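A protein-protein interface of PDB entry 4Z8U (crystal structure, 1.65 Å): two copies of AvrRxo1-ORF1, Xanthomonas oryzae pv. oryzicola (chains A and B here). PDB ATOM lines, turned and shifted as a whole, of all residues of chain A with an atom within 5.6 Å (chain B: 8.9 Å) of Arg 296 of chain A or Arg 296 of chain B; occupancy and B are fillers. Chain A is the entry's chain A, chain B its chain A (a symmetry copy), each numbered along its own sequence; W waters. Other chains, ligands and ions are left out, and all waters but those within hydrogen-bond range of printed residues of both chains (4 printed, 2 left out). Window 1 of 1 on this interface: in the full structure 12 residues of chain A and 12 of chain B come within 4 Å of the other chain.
NH1 of Arg 296 of chain A lies within salt-bridge range of OE1 of Glu 190 of chain A (2.9 Å). The side-chain carboxylate (OD2) of Asp 295 of chain A is in salt-bridge range of the side-chain amino group (NZ) of Lys 291 of chain A, 2.7 Å away. OE1 of Glu 190 of chain B is in salt-bridge range of NH1 of Arg 296 of chain B, at 2.9 Å. N of Glu 292 of chain B sits close to OD1 of Asp 290 of chain B. The backbone NH (N) of Leu 293 of chain B sits at hydrogen-bond distance from the side-chain carboxylate (OD1) of Asp 290 of chain B (2.9 Å). The side-chain carboxylate (OD2) of Asp 295 of chain B lies within salt-bridge range of the side-chain amino group (NZ) of Lys 291 of chain B, at 2.7 Å.
Water W3 lies within hydrogen-bond range of NZ of Lys 287 of chain A, OE1 of Glu 292 of chain A and ND2 of Asn 299 of chain B. Water W1 lies within hydrogen-bond range of NZ of Lys 287 of chain B, OD1 of Asp 290 of chain B, OE1 of Glu 292 of chain B and ND2 of Asn 299 of chain A. Water W2 lies within hydrogen-bond range of the side-chain amide oxygen of Asn 299 of chain B and the backbone NH of Glu 292 of chain A. Water W4 bridges the side-chain amide oxygen of Asn 299 of chain A (2.8 Å) and the backbone NH of Glu 292 of chain B (3.0 Å).
Of the 12 printed residues of chain A, 4 touch a printed residue of chain B. Of the 23 printed residues of chain B, 5 touch a printed residue of chain A. Among the printed residues, no Asp or Glu carboxylate lies within 4 Å of a Lys or Arg side-chain nitrogen of the other chain.
Glu 292 of chain B touches its own counterpart, Glu 292 of chain A. Glu 292 of chain A touches Arg 296 of chain B, and with the chains exchanged Arg 296 of chain A touches Glu 292 of chain B. Glu 292 of chain A touches Asn 299 of chain B, and with the chains exchanged Asn 299 of chain A touches Glu 292 of chain B. Arg 296 of chain A touches its own counterpart, Arg 296 of chain B. Of the 9 pairs that touch across the chains among the printed residues, 8 have their exchanged pair printed and touching as well.
Of the printed residues of chain B, Arg 296 of chain A touches Glu 292 (3.5 Å) and Arg 296 (3.99 Å). Printed residues of chain A within 4 Å of Arg 296 of chain B: Glu 292 (3.5 Å) and Arg 296 (3.99 Å). Printed residues of chain A within 4 Å of Glu 292 of chain B: Glu 292 (2.6 Å), Asp 295 (3.9 Å), Arg 296 (3.5 Å) and Asn 299 (3.5 Å). Printed residues of chain A within 4 Å of Asp 295 of chain B: Glu 292 (3.9 Å). Trp 322 of chain B touches none of the printed residues of chain A.
Among the printed residues, pairs that only touch across the chains: Arg 296 of chain A with Glu 292 of chain B (3.5 Å), Glu 292 of chain A with Arg 296 of chain B (3.5 Å), Glu 292 of chain A with Asn 299 of chain B (3.5 Å), Asn 299 of chain A with Glu 292 of chain B (3.5 Å), Asn 299 of chain A with Asp 290 of chain B (3.6 Å), Asp 295 of chain A with Glu 292 of chain B (3.9 Å), Glu 292 of chain A with Asp 295 of chain B (3.9 Å) and Arg 296 of chain A with Arg 296 of chain B (3.99 Å).
The side-chain carboxylate (OE2) of Glu 292 of chain B sits close to the side-chain carboxylate (OE2) of Glu 292 of chain A, at 2.6 Å.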
ATOM      1  N   GLU A 190       1.821   3.137  20.082  1.00  0.00           N
ATOM      2  CA  GLU A 190       2.770   2.992  18.940  1.00  0.00           C
ATOM      3  C   GLU A 190       3.622   1.780  19.066  1.00  0.00           C
ATOM      4  O   GLU A 190       4.027   1.164  18.034  1.00  0.00           O
ATOM      5  CB  GLU A 190       3.707   4.239  18.797  1.00  0.00           C
ATOM      6  CG  GLU A 190       3.148   5.158  17.819  1.00  0.00           C
ATOM      7  CD  GLU A 190       4.202   6.241  17.376  1.00  0.00           C
ATOM      8  OE1 GLU A 190       5.121   6.552  18.227  1.00  0.00           O
ATOM      9  OE2 GLU A 190       4.054   6.776  16.232  1.00  0.00           O
ATOM     10  N   LYS A 287      -0.771   9.101  10.864  1.00  0.00           N
ATOM     11  CA  LYS A 287       0.666   9.396  10.916  1.00  0.00           C
ATOM     12  C   LYS A 287       1.441   8.559   9.910  1.00  0.00           C
ATOM     13  O   LYS A 287       1.239   7.345   9.803  1.00  0.00           O
ATOM     14  CB  LYS A 287       1.191   9.250  12.345  1.00  0.00           C
ATOM     15  CG  LYS A 287       2.703   9.385  12.454  1.00  0.00           C
ATOM     16  CD  LYS A 287       3.201  10.766  12.068  1.00  0.00           C
ATOM     17  CE  LYS A 287       4.743  10.747  12.007  1.00  0.00           C
ATOM     18  NZ  LYS A 287       5.307  12.136  11.779  1.00  0.00           N
ATOM     19  N   LYS A 291      11.298   8.451   7.598  1.00  0.00           N
ATOM     20  CA  LYS A 291      12.626   8.181   8.173  1.00  0.00           C
ATOM     21  C   LYS A 291      12.691   8.620   9.667  1.00  0.00           C
ATOM     22  O   LYS A 291      13.161   7.911  10.523  1.00  0.00           O
ATOM     23  CB  LYS A 291      13.734   8.930   7.372  1.00  0.00           C
ATOM     24  CG  LYS A 291      15.163   8.634   7.853  1.00  0.00           C
ATOM     25  CD  LYS A 291      16.166   9.502   7.074  1.00  0.00           C
ATOM     26  CE  LYS A 291      17.603   9.384   7.610  1.00  0.00           C
ATOM     27  NZ  LYS A 291      17.601  10.007   8.948  1.00  0.00           N
ATOM     28  N   GLU A 292      12.213   9.795   9.945  1.00  0.00           N
ATOM     29  CA  GLU A 292      12.340  10.295  11.287  1.00  0.00           C
ATOM     30  C   GLU A 292      11.537   9.455  12.276  1.00  0.00           C
ATOM     31  O   GLU A 292      12.049   9.237  13.374  1.00  0.00           O
ATOM     32  CB  GLU A 292      11.880  11.727  11.397  1.00  0.00           C
ATOM     33  CG  GLU A 292      12.305  12.318  12.754  1.00  0.00           C
ATOM     34  CD  GLU A 292      11.278  12.007  13.848  1.00  0.00           C
ATOM     35  OE1 GLU A 292      10.035  12.066  13.530  1.00  0.00           O
ATOM     36  OE2 GLU A 292      11.732  11.738  15.002  1.00  0.00           O
ATOM     37  N   LEU A 293      10.335   9.027  11.889  1.00  0.00           N
ATOM     38  CA  LEU A 293       9.548   8.110  12.796  1.00  0.00           C
ATOM     39  C   LEU A 293      10.355   6.850  13.031  1.00  0.00           C
ATOM     40  O   LEU A 293      10.514   6.393  14.187  1.00  0.00           O
ATOM     41  CB  LEU A 293       8.177   7.738  12.200  1.00  0.00           C
ATOM     42  CG  LEU A 293       7.321   6.770  13.055  1.00  0.00           C
ATOM     43  CD1 LEU A 293       5.813   7.088  12.821  1.00  0.00           C
ATOM     44  CD2 LEU A 293       7.516   5.305  12.689  1.00  0.00           C
ATOM     45  N   ILE A 294      10.879   6.253  11.935  1.00  0.00           N
ATOM     46  CA  ILE A 294      11.773   5.084  12.162  1.00  0.00           C
ATOM     47  C   ILE A 294      12.982   5.348  13.068  1.00  0.00           C
ATOM     48  O   ILE A 294      13.229   4.592  13.975  1.00  0.00           O
ATOM     49  CB  ILE A 294      12.173   4.438  10.857  1.00  0.00           C
ATOM     50  CG1 ILE A 294      10.882   4.102  10.034  1.00  0.00           C
ATOM     51  CG2 ILE A 294      13.069   3.250  11.098  1.00  0.00           C
ATOM     52  CD1 ILE A 294      11.168   3.595   8.608  1.00  0.00           C
ATOM     53  N   ASP A 295      13.620   6.507  12.881  1.00  0.00           N
ATOM     54  CA  ASP A 295      14.753   6.925  13.721  1.00  0.00           C
ATOM     55  C   ASP A 295      14.223   7.244  15.120  1.00  0.00           C
ATOM     56  O   ASP A 295      14.933   6.969  16.034  1.00  0.00           O
ATOM     57  CB  ASP A 295      15.423   8.205  13.170  1.00  0.00           C
ATOM     58  CG  ASP A 295      16.206   7.937  11.855  1.00  0.00           C
ATOM     59  OD1 ASP A 295      16.432   6.738  11.478  1.00  0.00           O
ATOM     60  OD2 ASP A 295      16.587   8.948  11.215  1.00  0.00           O
ATOM     61  N   ARG A 296      13.028   7.825  15.253  1.00  0.00           N
ATOM     62  CA  ARG A 296      12.528   8.221  16.587  1.00  0.00           C
ATOM     63  C   ARG A 296      12.302   6.954  17.407  1.00  0.00           C
ATOM     64  O   ARG A 296      12.687   6.919  18.581  1.00  0.00           O
ATOM     65  CB  ARG A 296      11.268   9.047  16.531  1.00  0.00           C
ATOM     66  CG  ARG A 296      10.662   9.423  17.889  1.00  0.00           C
ATOM     67  CD  ARG A 296       9.447  10.322  17.727  1.00  0.00           C
ATOM     68  NE  ARG A 296       8.392   9.947  16.767  1.00  0.00           N
ATOM     69  CZ  ARG A 296       7.362   9.089  17.007  1.00  0.00           C
ATOM     70  NH1 ARG A 296       7.267   8.432  18.150  1.00  0.00           N
ATOM     71  NH2 ARG A 296       6.422   8.851  16.088  1.00  0.00           N
ATOM     72  N   LEU A 297      11.724   5.906  16.793  1.00  0.00           N
ATOM     73  CA  LEU A 297      11.598   4.615  17.467  1.00  0.00           C
ATOM     74  C   LEU A 297      12.868   3.896  17.719  1.00  0.00           C
ATOM     75  O   LEU A 297      13.055   3.314  18.824  1.00  0.00           O
ATOM     76  CB  LEU A 297      10.581   3.697  16.827  1.00  0.00           C
ATOM     77  CG  LEU A 297       9.189   4.334  16.726  1.00  0.00           C
ATOM     78  CD1 LEU A 297       8.295   3.432  15.904  1.00  0.00           C
ATOM     79  CD2 LEU A 297       8.523   4.587  18.090  1.00  0.00           C
ATOM     80  N   GLU A 298      13.751   3.878  16.719  1.00  0.00           N
ATOM     81  CA  GLU A 298      15.068   3.320  16.912  1.00  0.00           C
ATOM     82  C   GLU A 298      15.883   3.982  18.058  1.00  0.00           C
ATOM     83  O   GLU A 298      16.739   3.328  18.663  1.00  0.00           O
ATOM     84  CB  GLU A 298      15.888   3.410  15.601  1.00  0.00           C
ATOM     85  CG  GLU A 298      15.359   2.536  14.512  1.00  0.00           C
ATOM     86  CD  GLU A 298      15.694   1.082  14.747  1.00  0.00           C
ATOM     87  OE1 GLU A 298      16.907   0.693  14.646  1.00  0.00           O
ATOM     88  OE2 GLU A 298      14.726   0.323  15.008  1.00  0.00           O
ATOM     89  N   ASN A 299      15.697   5.303  18.272  1.00  0.00           N
ATOM     90  CA  ASN A 299      16.503   6.040  19.288  1.00  0.00           C
ATOM     91  C   ASN A 299      16.314   5.497  20.687  1.00  0.00           C
ATOM     92  O   ASN A 299      17.191   5.676  21.578  1.00  0.00           O
ATOM     93  CB  ASN A 299      16.088   7.525  19.280  1.00  0.00           C
ATOM     94  CG  ASN A 299      17.077   8.423  19.983  1.00  0.00           C
ATOM     95  OD1 ASN A 299      18.283   8.355  19.739  1.00  0.00           O
ATOM     96  ND2 ASN A 299      16.574   9.277  20.872  1.00  0.00           N
ATOM     97  N   ASN A 300      15.151   4.845  20.908  1.00  0.00           N
ATOM     98  CA  ASN A 300      14.839   4.264  22.215  1.00  0.00           C
ATOM     99  C   ASN A 300      14.885   2.789  22.252  1.00  0.00           C
ATOM    100  O   ASN A 300      14.308   2.133  23.151  1.00  0.00           O
ATOM    101  CB  ASN A 300      13.491   4.772  22.754  1.00  0.00           C
ATOM    102  CG  ASN A 300      13.474   6.271  22.963  1.00  0.00           C
ATOM    103  OD1 ASN A 300      12.639   6.992  22.394  1.00  0.00           O
ATOM    104  ND2 ASN A 300      14.342   6.740  23.800  1.00  0.00           N
ATOM    105  N   PRO B 188       4.115  25.101  21.653  1.00  0.00           N
ATOM    106  CA  PRO B 188       4.522  24.048  22.606  1.00  0.00           C
ATOM    107  C   PRO B 188       5.789  24.483  23.331  1.00  0.00           C
ATOM    108  O   PRO B 188       6.595  25.285  22.824  1.00  0.00           O
ATOM    109  CB  PRO B 188       4.816  22.811  21.671  1.00  0.00           C
ATOM    110  CG  PRO B 188       4.051  23.109  20.387  1.00  0.00           C
ATOM    111  CD  PRO B 188       4.042  24.618  20.245  1.00  0.00           C
ATOM    112  N   GLU B 190       8.506  22.990  23.971  1.00  0.00           N
ATOM    113  CA  GLU B 190       9.807  22.736  23.289  1.00  0.00           C
ATOM    114  C   GLU B 190      10.099  23.744  22.235  1.00  0.00           C
ATOM    115  O   GLU B 190      11.294  24.076  21.971  1.00  0.00           O
ATOM    116  CB  GLU B 190       9.855  21.314  22.634  1.00  0.00           C
ATOM    117  CG  GLU B 190      10.497  20.380  23.545  1.00  0.00           C
ATOM    118  CD  GLU B 190      10.889  19.040  22.816  1.00  0.00           C
ATOM    119  OE1 GLU B 190      10.176  18.692  21.798  1.00  0.00           O
ATOM    120  OE2 GLU B 190      11.847  18.361  23.303  1.00  0.00           O
ATOM    121  N   ASN B 191       9.075  24.246  21.550  1.00  0.00           N
ATOM    122  CA  ASN B 191       9.287  25.341  20.562  1.00  0.00           C
ATOM    123  C   ASN B 191       9.825  26.613  21.201  1.00  0.00           C
ATOM    124  O   ASN B 191      10.676  27.270  20.654  1.00  0.00           O
ATOM    125  CB  ASN B 191       7.940  25.698  19.835  1.00  0.00           C
ATOM    126  CG  ASN B 191       7.546  24.632  18.808  1.00  0.00           C
ATOM    127  OD1 ASN B 191       7.704  23.468  19.040  1.00  0.00           O
ATOM    128  ND2 ASN B 191       6.952  25.067  17.676  1.00  0.00           N
ATOM    129  N   GLU B 247       1.436  21.423  13.735  1.00  0.00           N
ATOM    130  CA  GLU B 247       2.563  20.492  13.748  1.00  0.00           C
ATOM    131  C   GLU B 247       3.690  20.977  12.871  1.00  0.00           C
ATOM    132  O   GLU B 247       4.859  20.731  13.186  1.00  0.00           O
ATOM    133  CB  GLU B 247       2.114  19.126  13.298  1.00  0.00           C
ATOM    134  CG  GLU B 247       0.998  18.623  14.189  1.00  0.00           C
ATOM    135  CD  GLU B 247      -0.387  19.065  13.700  1.00  0.00           C
ATOM    136  OE1 GLU B 247      -0.653  20.331  13.529  1.00  0.00           O
ATOM    137  OE2 GLU B 247      -1.223  18.116  13.499  1.00  0.00           O
ATOM    138  N   LEU B 284      10.813  17.448  31.159  1.00  0.00           N
ATOM    139  CA  LEU B 284      11.438  17.808  29.925  1.00  0.00           C
ATOM    140  C   LEU B 284      12.809  18.487  30.217  1.00  0.00           C
ATOM    141  O   LEU B 284      13.684  18.558  29.308  1.00  0.00           O
ATOM    142  CB  LEU B 284      10.510  18.812  29.223  1.00  0.00           C
ATOM    143  CG  LEU B 284      10.860  19.251  27.855  1.00  0.00           C
ATOM    144  CD1 LEU B 284      10.837  18.099  26.835  1.00  0.00           C
ATOM    145  CD2 LEU B 284       9.967  20.426  27.348  1.00  0.00           C
ATOM    146  N   LYS B 287      15.622  16.222  29.521  1.00  0.00           N
ATOM    147  CA  LYS B 287      15.775  15.644  28.181  1.00  0.00           C
ATOM    148  C   LYS B 287      17.060  16.115  27.517  1.00  0.00           C
ATOM    149  O   LYS B 287      17.380  17.308  27.528  1.00  0.00           O
ATOM    150  CB  LYS B 287      14.530  15.918  27.335  1.00  0.00           C
ATOM    151  CG  LYS B 287      14.676  15.488  25.883  1.00  0.00           C
ATOM    152  CD  LYS B 287      14.847  13.989  25.726  1.00  0.00           C
ATOM    153  CE  LYS B 287      15.193  13.672  24.255  1.00  0.00           C
ATOM    154  NZ  LYS B 287      15.224  12.177  24.002  1.00  0.00           N
ATOM    155  N   VAL B 288      17.840  15.172  26.973  1.00  0.00           N
ATOM    156  CA  VAL B 288      19.131  15.566  26.421  1.00  0.00           C
ATOM    157  C   VAL B 288      18.982  15.906  24.928  1.00  0.00           C
ATOM    158  O   VAL B 288      18.332  15.197  24.111  1.00  0.00           O
ATOM    159  CB  VAL B 288      20.148  14.393  26.658  1.00  0.00           C
ATOM    160  CG1 VAL B 288      21.423  14.688  25.851  1.00  0.00           C
ATOM    161  CG2 VAL B 288      20.457  14.259  28.142  1.00  0.00           C
ATOM    162  N   ILE B 289      19.568  17.021  24.526  1.00  0.00           N
ATOM    163  CA  ILE B 289      19.616  17.390  23.084  1.00  0.00           C
ATOM    164  C   ILE B 289      20.581  16.482  22.321  1.00  0.00           C
ATOM    165  O   ILE B 289      21.824  16.668  22.453  1.00  0.00           O
ATOM    166  CB  ILE B 289      20.114  18.809  22.944  1.00  0.00           C
ATOM    167  CG1 ILE B 289      19.175  19.731  23.690  1.00  0.00           C
ATOM    168  CG2 ILE B 289      20.265  19.231  21.456  1.00  0.00           C
ATOM    169  CD1 ILE B 289      19.661  21.194  23.763  1.00  0.00           C
ATOM    170  N   ASP B 290      20.035  15.519  21.585  1.00  0.00           N
ATOM    171  CA  ASP B 290      20.856  14.576  20.807  1.00  0.00           C
ATOM    172  C   ASP B 290      20.477  14.588  19.362  1.00  0.00           C
ATOM    173  O   ASP B 290      19.636  15.392  18.940  1.00  0.00           O
ATOM    174  CB  ASP B 290      20.767  13.156  21.377  1.00  0.00           C
ATOM    175  CG  ASP B 290      19.327  12.599  21.420  1.00  0.00           C
ATOM    176  OD1 ASP B 290      18.388  13.101  20.776  1.00  0.00           O
ATOM    177  OD2 ASP B 290      19.111  11.552  22.058  1.00  0.00           O
ATOM    178  N   LYS B 291      21.118  13.748  18.548  1.00  0.00           N
ATOM    179  CA  LYS B 291      20.866  13.826  17.098  1.00  0.00           C
ATOM    180  C   LYS B 291      19.352  13.646  16.780  1.00  0.00           C
ATOM    181  O   LYS B 291      18.765  14.375  16.018  1.00  0.00           O
ATOM    182  CB  LYS B 291      21.682  12.735  16.341  1.00  0.00           C
ATOM    183  CG  LYS B 291      21.546  12.801  14.812  1.00  0.00           C
ATOM    184  CD  LYS B 291      22.295  11.622  14.169  1.00  0.00           C
ATOM    185  CE  LYS B 291      22.070  11.524  12.651  1.00  0.00           C
ATOM    186  NZ  LYS B 291      20.654  11.153  12.463  1.00  0.00           N
ATOM    187  N   GLU B 292      18.750  12.662  17.379  1.00  0.00           N
ATOM    188  CA  GLU B 292      17.379  12.383  17.044  1.00  0.00           C
ATOM    189  C   GLU B 292      16.459  13.530  17.453  1.00  0.00           C
ATOM    190  O   GLU B 292      15.544  13.819  16.680  1.00  0.00           O
ATOM    191  CB  GLU B 292      16.887  11.121  17.705  1.00  0.00           C
ATOM    192  CG  GLU B 292      15.538  10.694  17.098  1.00  0.00           C
ATOM    193  CD  GLU B 292      14.364  11.397  17.788  1.00  0.00           C
ATOM    194  OE1 GLU B 292      14.428  11.547  19.062  1.00  0.00           O
ATOM    195  OE2 GLU B 292      13.396  11.757  17.051  1.00  0.00           O
ATOM    196  N   LEU B 293      16.699  14.129  18.620  1.00  0.00           N
ATOM    197  CA  LEU B 293      15.877  15.333  19.018  1.00  0.00           C
ATOM    198  C   LEU B 293      16.065  16.416  17.976  1.00  0.00           C
ATOM    199  O   LEU B 293      15.081  17.020  17.489  1.00  0.00           O
ATOM    200  CB  LEU B 293      16.274  15.878  20.402  1.00  0.00           C
ATOM    201  CG  LEU B 293      15.500  17.135  20.868  1.00  0.00           C
ATOM    202  CD1 LEU B 293      15.380  17.108  22.423  1.00  0.00           C
ATOM    203  CD2 LEU B 293      16.196  18.442  20.513  1.00  0.00           C
ATOM    204  N   ILE B 294      17.339  16.692  17.612  1.00  0.00           N
ATOM    205  CA  ILE B 294      17.533  17.668  16.506  1.00  0.00           C
ATOM    206  C   ILE B 294      16.829  17.313  15.188  1.00  0.00           C
ATOM    207  O   ILE B 294      16.164  18.145  14.621  1.00  0.00           O
ATOM    208  CB  ILE B 294      18.995  17.983  16.300  1.00  0.00           C
ATOM    209  CG1 ILE B 294      19.618  18.437  17.664  1.00  0.00           C
ATOM    210  CG2 ILE B 294      19.179  18.979  15.184  1.00  0.00           C
ATOM    211  CD1 ILE B 294      21.147  18.622  17.619  1.00  0.00           C
ATOM    212  N   ASP B 295      16.882  16.032  14.815  1.00  0.00           N
ATOM    213  CA  ASP B 295      16.197  15.535  13.613  1.00  0.00           C
ATOM    214  C   ASP B 295      14.689  15.578  13.866  1.00  0.00           C
ATOM    215  O   ASP B 295      14.000  15.850  12.935  1.00  0.00           O
ATOM    216  CB  ASP B 295      16.580  14.068  13.310  1.00  0.00           C
ATOM    217  CG  ASP B 295      18.043  13.936  12.805  1.00  0.00           C
ATOM    218  OD1 ASP B 295      18.699  14.978  12.467  1.00  0.00           O
ATOM    219  OD2 ASP B 295      18.514  12.773  12.753  1.00  0.00           O
ATOM    220  N   ARG B 296      14.218  15.293  15.083  1.00  0.00           N
ATOM    221  CA  ARG B 296      12.762  15.245  15.335  1.00  0.00           C
ATOM    222  C   ARG B 296      12.200  16.653  15.153  1.00  0.00           C
ATOM    223  O   ARG B 296      11.152  16.806  14.518  1.00  0.00           O
ATOM    224  CB  ARG B 296      12.409  14.706  16.698  1.00  0.00           C
ATOM    225  CG  ARG B 296      10.915  14.703  17.043  1.00  0.00           C
ATOM    226  CD  ARG B 296      10.658  14.066  18.399  1.00  0.00           C
ATOM    227  NE  ARG B 296      11.465  14.486  19.561  1.00  0.00           N
ATOM    228  CZ  ARG B 296      11.225  15.570  20.350  1.00  0.00           C
ATOM    229  NH1 ARG B 296      10.248  16.418  20.075  1.00  0.00           N
ATOM    230  NH2 ARG B 296      11.984  15.840  21.414  1.00  0.00           N
ATOM    231  N   LEU B 297      12.904  17.678  15.666  1.00  0.00           N
ATOM    232  CA  LEU B 297      12.506  19.062  15.417  1.00  0.00           C
ATOM    233  C   LEU B 297      12.649  19.530  14.018  1.00  0.00           C
ATOM    234  O   LEU B 297      11.746  20.240  13.496  1.00  0.00           O
ATOM    235  CB  LEU B 297      13.126  20.051  16.378  1.00  0.00           C
ATOM    236  CG  LEU B 297      12.833  19.714  17.846  1.00  0.00           C
ATOM    237  CD1 LEU B 297      13.647  20.631  18.733  1.00  0.00           C
ATOM    238  CD2 LEU B 297      11.348  19.844  18.227  1.00  0.00           C
ATOM    239  N   GLU B 298      13.775  19.191  13.390  1.00  0.00           N
ATOM    240  CA  GLU B 298      13.951  19.484  11.988  1.00  0.00           C
ATOM    241  C   GLU B 298      12.861  18.870  11.065  1.00  0.00           C
ATOM    242  O   GLU B 298      12.576  19.423   9.997  1.00  0.00           O
ATOM    243  CB  GLU B 298      15.341  19.000  11.506  1.00  0.00           C
ATOM    244  CG  GLU B 298      16.473  19.766  12.106  1.00  0.00           C
ATOM    245  CD  GLU B 298      16.616  21.136  11.485  1.00  0.00           C
ATOM    246  OE1 GLU B 298      17.018  21.237  10.275  1.00  0.00           O
ATOM    247  OE2 GLU B 298      16.347  22.115  12.226  1.00  0.00           O
ATOM    248  N   ASN B 299      12.343  17.675  11.421  1.00  0.00           N
ATOM    249  CA  ASN B 299      11.361  16.969  10.548  1.00  0.00           C
ATOM    250  C   ASN B 299      10.097  17.770  10.327  1.00  0.00           C
ATOM    251  O   ASN B 299       9.366  17.565   9.317  1.00  0.00           O
ATOM    252  CB  ASN B 299      10.980  15.625  11.201  1.00  0.00           C
ATOM    253  CG  ASN B 299      10.297  14.673  10.250  1.00  0.00           C
ATOM    254  OD1 ASN B 299      10.768  14.442   9.133  1.00  0.00           O
ATOM    255  ND2 ASN B 299       9.171  14.108  10.681  1.00  0.00           N
ATOM    256  N   ASN B 300       9.808  18.680  11.282  1.00  0.00           N
ATOM    257  CA  ASN B 300       8.618  19.528  11.193  1.00  0.00           C
ATOM    258  C   ASN B 300       8.902  20.945  10.889  1.00  0.00           C
ATOM    259  O   ASN B 300       8.071  21.851  11.132  1.00  0.00           O
ATOM    260  CB  ASN B 300       7.746  19.415  12.455  1.00  0.00           C
ATOM    261  CG  ASN B 300       7.226  18.012  12.681  1.00  0.00           C
ATOM    262  OD1 ASN B 300       7.466  17.396  13.731  1.00  0.00           O
ATOM    263  ND2 ASN B 300       6.484  17.521  11.742  1.00  0.00           N
ATOM    264  N   ILE B 301      10.080  21.180  10.337  1.00  0.00           N
ATOM    265  CA  ILE B 301      10.409  22.549   9.923  1.00  0.00           C
ATOM    266  C   ILE B 301      10.827  22.508   8.413  1.00  0.00           C
ATOM    267  O   ILE B 301      11.939  22.025   8.073  1.00  0.00           O
ATOM    268  CB  ILE B 301      11.597  23.197  10.676  1.00  0.00           C
ATOM    269  CG1 ILE B 301      11.438  23.078  12.187  1.00  0.00           C
ATOM    270  CG2 ILE B 301      11.825  24.632  10.197  1.00  0.00           C
ATOM    271  CD1 ILE B 301      12.489  23.787  13.007  1.00  0.00           C
ATOM    272  N   THR B 310      17.672  26.758  13.538  1.00  0.00           N
ATOM    273  CA  THR B 310      17.283  25.826  14.595  1.00  0.00           C
ATOM    274  C   THR B 310      18.397  24.836  14.848  1.00  0.00           C
ATOM    275  O   THR B 310      18.848  24.599  15.958  1.00  0.00           O
ATOM    276  CB  THR B 310      15.952  25.151  14.241  1.00  0.00           C
ATOM    277  OG1 THR B 310      14.945  26.177  14.114  1.00  0.00           O
ATOM    278  CG2 THR B 310      15.466  24.102  15.301  1.00  0.00           C
ATOM    279  N   LEU B 314      20.751  24.313  18.287  1.00  0.00           N
ATOM    280  CA  LEU B 314      20.735  23.061  18.952  1.00  0.00           C
ATOM    281  C   LEU B 314      22.082  22.321  18.980  1.00  0.00           C
ATOM    282  O   LEU B 314      22.482  21.846  20.003  1.00  0.00           O
ATOM    283  CB  LEU B 314      19.664  22.157  18.414  1.00  0.00           C
ATOM    284  CG  LEU B 314      18.212  22.581  18.649  1.00  0.00           C
ATOM    285  CD1 LEU B 314      17.248  21.717  17.853  1.00  0.00           C
ATOM    286  CD2 LEU B 314      17.945  22.545  20.153  1.00  0.00           C
ATOM    287  N   TRP B 322      17.944  20.075  28.224  1.00  0.00           N
ATOM    288  CA  TRP B 322      17.398  21.396  27.929  1.00  0.00           C
ATOM    289  C   TRP B 322      17.730  22.374  29.034  1.00  0.00           C
ATOM    290  O   TRP B 322      17.981  23.540  28.795  1.00  0.00           O
ATOM    291  CB  TRP B 322      15.837  21.290  27.876  1.00  0.00           C
ATOM    292  CG  TRP B 322      15.239  20.778  26.624  1.00  0.00           C
ATOM    293  CD1 TRP B 322      14.415  19.671  26.447  1.00  0.00           C
ATOM    294  CD2 TRP B 322      15.354  21.378  25.317  1.00  0.00           C
ATOM    295  NE1 TRP B 322      13.987  19.601  25.185  1.00  0.00           N
ATOM    296  CE2 TRP B 322      14.530  20.561  24.425  1.00  0.00           C
ATOM    297  CE3 TRP B 322      16.014  22.500  24.817  1.00  0.00           C
ATOM    298  CZ2 TRP B 322      14.371  20.868  23.093  1.00  0.00           C
ATOM    299  CZ3 TRP B 322      15.842  22.825  23.459  1.00  0.00           C
ATOM    300  CH2 TRP B 322      15.058  22.011  22.604  1.00  0.00           C
HETATM  301  O   HOH W   1      15.824  12.324  21.496  1.00  0.00           O
HETATM  302  O   HOH W   2      11.495  12.014   8.020  1.00  0.00           O
HETATM  303  O   HOH W   3       7.793  11.440  11.783  1.00  0.00           O
HETATM  304  O   HOH W   4      19.999  10.349  18.873  1.00  0.00           O
